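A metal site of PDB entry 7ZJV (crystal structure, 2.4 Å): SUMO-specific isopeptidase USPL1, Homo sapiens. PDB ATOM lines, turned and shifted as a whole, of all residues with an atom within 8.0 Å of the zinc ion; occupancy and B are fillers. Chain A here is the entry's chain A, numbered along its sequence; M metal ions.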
ATOM      1  N   PHE A 144     -12.918   0.964 -18.424  1.00  0.00           N
ATOM      2  CA  PHE A 144     -12.449   0.497 -19.718  1.00  0.00           C
ATOM      3  C   PHE A 144     -12.962  -0.921 -19.939  1.00  0.00           C
ATOM      4  O   PHE A 144     -12.971  -1.735 -19.011  1.00  0.00           O
ATOM      5  CB  PHE A 144     -10.923   0.552 -19.763  1.00  0.00           C
ATOM      6  CG  PHE A 144     -10.330   0.097 -21.056  1.00  0.00           C
ATOM      7  CD1 PHE A 144     -10.113   1.002 -22.079  1.00  0.00           C
ATOM      8  CD2 PHE A 144      -9.967  -1.222 -21.253  1.00  0.00           C
ATOM      9  CE1 PHE A 144      -9.559   0.608 -23.275  1.00  0.00           C
ATOM     10  CE2 PHE A 144      -9.410  -1.630 -22.450  1.00  0.00           C
ATOM     11  CZ  PHE A 144      -9.209  -0.707 -23.469  1.00  0.00           C
ATOM     12  N   GLU A 145     -13.284  -1.228 -21.194  1.00  0.00           N
ATOM     13  CA  GLU A 145     -13.740  -2.565 -21.587  1.00  0.00           C
ATOM     14  C   GLU A 145     -13.472  -2.707 -23.075  1.00  0.00           C
ATOM     15  O   GLU A 145     -14.155  -2.074 -23.897  1.00  0.00           O
ATOM     16  CB  GLU A 145     -15.224  -2.756 -21.260  1.00  0.00           C
ATOM     17  CG  GLU A 145     -15.794  -4.085 -21.765  1.00  0.00           C
ATOM     18  CD  GLU A 145     -17.154  -4.416 -21.155  1.00  0.00           C
ATOM     19  OE1 GLU A 145     -17.269  -5.486 -20.510  1.00  0.00           O
ATOM     20  OE2 GLU A 145     -18.092  -3.613 -21.314  1.00  0.00           O
ATOM     21  N   CYS A 146     -12.496  -3.545 -23.428  1.00  0.00           N
ATOM     22  CA  CYS A 146     -12.148  -3.736 -24.837  1.00  0.00           C
ATOM     23  C   CYS A 146     -13.214  -4.547 -25.555  1.00  0.00           C
ATOM     24  O   CYS A 146     -13.780  -5.502 -25.000  1.00  0.00           O
ATOM     25  CB  CYS A 146     -10.799  -4.454 -24.938  1.00  0.00           C
ATOM     26  SG  CYS A 146     -10.209  -4.763 -26.613  1.00  0.00           S
ATOM     27  N   SER A 147     -13.543  -4.124 -26.782  1.00  0.00           N
ATOM     28  CA  SER A 147     -14.485  -4.869 -27.602  1.00  0.00           C
ATOM     29  C   SER A 147     -13.854  -5.954 -28.477  1.00  0.00           C
ATOM     30  O   SER A 147     -14.564  -6.872 -28.886  1.00  0.00           O
ATOM     31  CB  SER A 147     -15.260  -3.892 -28.503  1.00  0.00           C
ATOM     32  OG  SER A 147     -14.517  -3.579 -29.667  1.00  0.00           O
ATOM     33  N   GLN A 148     -12.560  -5.879 -28.778  1.00  0.00           N
ATOM     34  CA  GLN A 148     -11.962  -6.925 -29.605  1.00  0.00           C
ATOM     35  C   GLN A 148     -11.670  -8.147 -28.755  1.00  0.00           C
ATOM     36  O   GLN A 148     -12.122  -9.260 -29.051  1.00  0.00           O
ATOM     37  CB  GLN A 148     -10.678  -6.423 -30.273  1.00  0.00           C
ATOM     38  N   CYS A 149     -10.930  -7.951 -27.668  1.00  0.00           N
ATOM     39  CA  CYS A 149     -10.724  -8.960 -26.656  1.00  0.00           C
ATOM     40  C   CYS A 149     -11.472  -8.489 -25.421  1.00  0.00           C
ATOM     41  O   CYS A 149     -12.172  -7.482 -25.442  1.00  0.00           O
ATOM     42  CB  CYS A 149      -9.235  -9.157 -26.362  1.00  0.00           C
ATOM     43  SG  CYS A 149      -8.433  -7.760 -25.541  1.00  0.00           S
ATOM     44  N   GLY A 150     -11.315  -9.231 -24.354  1.00  0.00           N
ATOM     45  CA  GLY A 150     -11.972  -8.959 -23.099  1.00  0.00           C
ATOM     46  C   GLY A 150     -11.311  -8.030 -22.108  1.00  0.00           C
ATOM     47  O   GLY A 150     -11.865  -7.874 -21.010  1.00  0.00           O
ATOM     48  N   HIS A 151     -10.164  -7.441 -22.417  1.00  0.00           N
ATOM     49  CA  HIS A 151      -9.409  -6.736 -21.386  1.00  0.00           C
ATOM     50  C   HIS A 151     -10.309  -5.648 -20.822  1.00  0.00           C
ATOM     51  O   HIS A 151     -10.869  -4.837 -21.562  1.00  0.00           O
ATOM     52  CB  HIS A 151      -8.110  -6.168 -21.953  1.00  0.00           C
ATOM     53  CG  HIS A 151      -7.254  -5.468 -20.936  1.00  0.00           C
ATOM     54  ND1 HIS A 151      -6.689  -6.130 -19.866  1.00  0.00           N
ATOM     55  CD2 HIS A 151      -6.828  -4.178 -20.858  1.00  0.00           C
ATOM     56  CE1 HIS A 151      -5.979  -5.278 -19.157  1.00  0.00           C
ATOM     57  NE2 HIS A 151      -6.042  -4.093 -19.739  1.00  0.00           N
ATOM     58  N   GLN A 152     -10.428  -5.618 -19.493  1.00  0.00           N
ATOM     59  CA  GLN A 152     -11.302  -4.656 -18.854  1.00  0.00           C
ATOM     60  C   GLN A 152     -10.754  -4.230 -17.502  1.00  0.00           C
ATOM     61  O   GLN A 152     -10.047  -4.988 -16.838  1.00  0.00           O
ATOM     62  CB  GLN A 152     -12.642  -5.395 -18.697  1.00  0.00           C
ATOM     63  CG  GLN A 152     -13.926  -4.676 -18.395  1.00  0.00           C
ATOM     64  CD  GLN A 152     -15.069  -5.682 -18.267  1.00  0.00           C
ATOM     65  OE1 GLN A 152     -15.042  -6.740 -18.899  1.00  0.00           O
ATOM     66  NE2 GLN A 152     -16.054  -5.366 -17.440  1.00  0.00           N
ATOM     67  N   PRO A 181      -5.918   3.025 -26.982  1.00  0.00           N
ATOM     68  CA  PRO A 181      -5.572   1.646 -27.344  1.00  0.00           C
ATOM     69  C   PRO A 181      -5.849   0.714 -26.180  1.00  0.00           C
ATOM     70  O   PRO A 181      -6.010   1.117 -25.035  1.00  0.00           O
ATOM     71  CB  PRO A 181      -4.072   1.719 -27.624  1.00  0.00           C
ATOM     72  CG  PRO A 181      -3.594   2.846 -26.756  1.00  0.00           C
ATOM     73  CD  PRO A 181      -4.727   3.830 -26.669  1.00  0.00           C
ATOM     74  N   CYS A 182      -5.913  -0.583 -26.506  1.00  0.00           N
ATOM     75  CA  CYS A 182      -6.084  -1.600 -25.492  1.00  0.00           C
ATOM     76  C   CYS A 182      -4.705  -2.166 -25.160  1.00  0.00           C
ATOM     77  O   CYS A 182      -3.968  -2.565 -26.056  1.00  0.00           O
ATOM     78  CB  CYS A 182      -7.022  -2.714 -25.951  1.00  0.00           C
ATOM     79  SG  CYS A 182      -6.969  -4.181 -24.902  1.00  0.00           S
ATOM     80  N   ASN A 183      -4.380  -2.203 -23.871  1.00  0.00           N
ATOM     81  CA  ASN A 183      -3.083  -2.669 -23.414  1.00  0.00           C
ATOM     82  C   ASN A 183      -2.890  -4.175 -23.558  1.00  0.00           C
ATOM     83  O   ASN A 183      -1.767  -4.656 -23.393  1.00  0.00           O
ATOM     84  CB  ASN A 183      -2.825  -2.182 -21.986  1.00  0.00           C
ATOM     85  CG  ASN A 183      -2.733  -0.666 -21.907  1.00  0.00           C
ATOM     86  OD1 ASN A 183      -2.109  -0.031 -22.774  1.00  0.00           O
ATOM     87  ND2 ASN A 183      -3.355  -0.080 -20.898  1.00  0.00           N
ATOM     88  N   ASN A 184      -3.952  -4.928 -23.828  1.00  0.00           N
ATOM     89  CA  ASN A 184      -3.866  -6.385 -23.894  1.00  0.00           C
ATOM     90  C   ASN A 184      -3.622  -6.881 -25.315  1.00  0.00           C
ATOM     91  O   ASN A 184      -2.898  -7.861 -25.518  1.00  0.00           O
ATOM     92  CB  ASN A 184      -5.128  -7.025 -23.332  1.00  0.00           C
ATOM     93  N   CYS A 185      -4.230  -6.229 -26.304  1.00  0.00           N
ATOM     94  CA  CYS A 185      -4.142  -6.668 -27.686  1.00  0.00           C
ATOM     95  C   CYS A 185      -3.669  -5.610 -28.677  1.00  0.00           C
ATOM     96  O   CYS A 185      -3.656  -5.878 -29.885  1.00  0.00           O
ATOM     97  CB  CYS A 185      -5.514  -7.216 -28.125  1.00  0.00           C
ATOM     98  SG  CYS A 185      -6.777  -5.937 -28.291  1.00  0.00           S
ATOM     99  N   ASN A 186      -3.310  -4.410 -28.209  1.00  0.00           N
ATOM    100  CA  ASN A 186      -2.779  -3.326 -29.037  1.00  0.00           C
ATOM    101  C   ASN A 186      -3.771  -2.880 -30.101  1.00  0.00           C
ATOM    102  O   ASN A 186      -3.403  -2.197 -31.061  1.00  0.00           O
ATOM    103  CB  ASN A 186      -1.443  -3.724 -29.681  1.00  0.00           C
ATOM    104  CG  ASN A 186      -0.510  -2.550 -29.895  1.00  0.00           C
ATOM    105  OD1 ASN A 186      -0.768  -1.446 -29.425  1.00  0.00           O
ATOM    106  ND2 ASN A 186       0.597  -2.788 -30.589  1.00  0.00           N
ATOM    107  N   SER A 187      -5.030  -3.222 -29.893  1.00  0.00           N
ATOM    108  CA  SER A 187      -6.130  -2.730 -30.704  1.00  0.00           C
ATOM    109  C   SER A 187      -6.371  -1.263 -30.416  1.00  0.00           C
ATOM    110  O   SER A 187      -6.318  -0.821 -29.276  1.00  0.00           O
ATOM    111  CB  SER A 187      -7.411  -3.515 -30.470  1.00  0.00           C
ATOM    112  OG  SER A 187      -8.512  -2.645 -30.343  1.00  0.00           O
ATOM    113  N   LYS A 188      -6.637  -0.517 -31.472  1.00  0.00           N
ATOM    114  CA  LYS A 188      -6.889   0.906 -31.343  1.00  0.00           C
ATOM    115  C   LYS A 188      -8.405   1.091 -31.283  1.00  0.00           C
ATOM    116  O   LYS A 188      -9.180   0.164 -31.526  1.00  0.00           O
ATOM    117  CB  LYS A 188      -6.274   1.691 -32.496  1.00  0.00           C
ATOM    118  N   GLN A 190     -10.442   1.468 -28.742  1.00  0.00           N
ATOM    119  CA  GLN A 190     -11.337   1.243 -27.620  1.00  0.00           C
ATOM    120  C   GLN A 190     -11.557   2.570 -26.900  1.00  0.00           C
ATOM    121  O   GLN A 190     -10.940   3.585 -27.225  1.00  0.00           O
ATOM    122  CB  GLN A 190     -10.856   0.103 -26.740  1.00  0.00           C
ATOM    123  CG  GLN A 190     -10.700  -1.124 -27.584  1.00  0.00           C
ATOM    124  CD  GLN A 190     -12.084  -1.617 -28.017  1.00  0.00           C
ATOM    125  OE1 GLN A 190     -13.050  -1.506 -27.271  1.00  0.00           O
ATOM    126  NE2 GLN A 190     -12.185  -2.119 -29.242  1.00  0.00           N
HETATM  127 ZN    ZN M   1      -8.062  -5.626 -26.385  1.00  0.00          ZN
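SG of Cys 185 is bound to the zinc ion, 2.3 Å away. SG of Cys 149 binds the zinc ion (2.3 Å). SG of Cys 146 binds the zinc ion (2.3 Å). The zinc ion is bound by SG of Cys 182, at 2.3 Å. The zinc ion has four donor atoms within binding distance.
The nearest printed residue that does not touch the zinc ion is Asn 184 (4.5 Å).
SG of Cys 185 sits close to N of Ser 187, at 3.6 Å. The backbone NH of Gln 148 lies close to the side-chain sulfur of Cys 146, at 3.4 Å. N of Asn 184 sits close to SG of Cys 182, 3.3 Å away. N of His 151 sits close to SG of Cys 149 (3.6 Å). The backbone NH (N) of Cys 182 is in hydrogen-bond range of the backbone carbonyl oxygen (O) of Ser 187 (2.8 Å). N of Cys 146 sits at hydrogen-bond distance from O of His 151 (2.8 Å).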
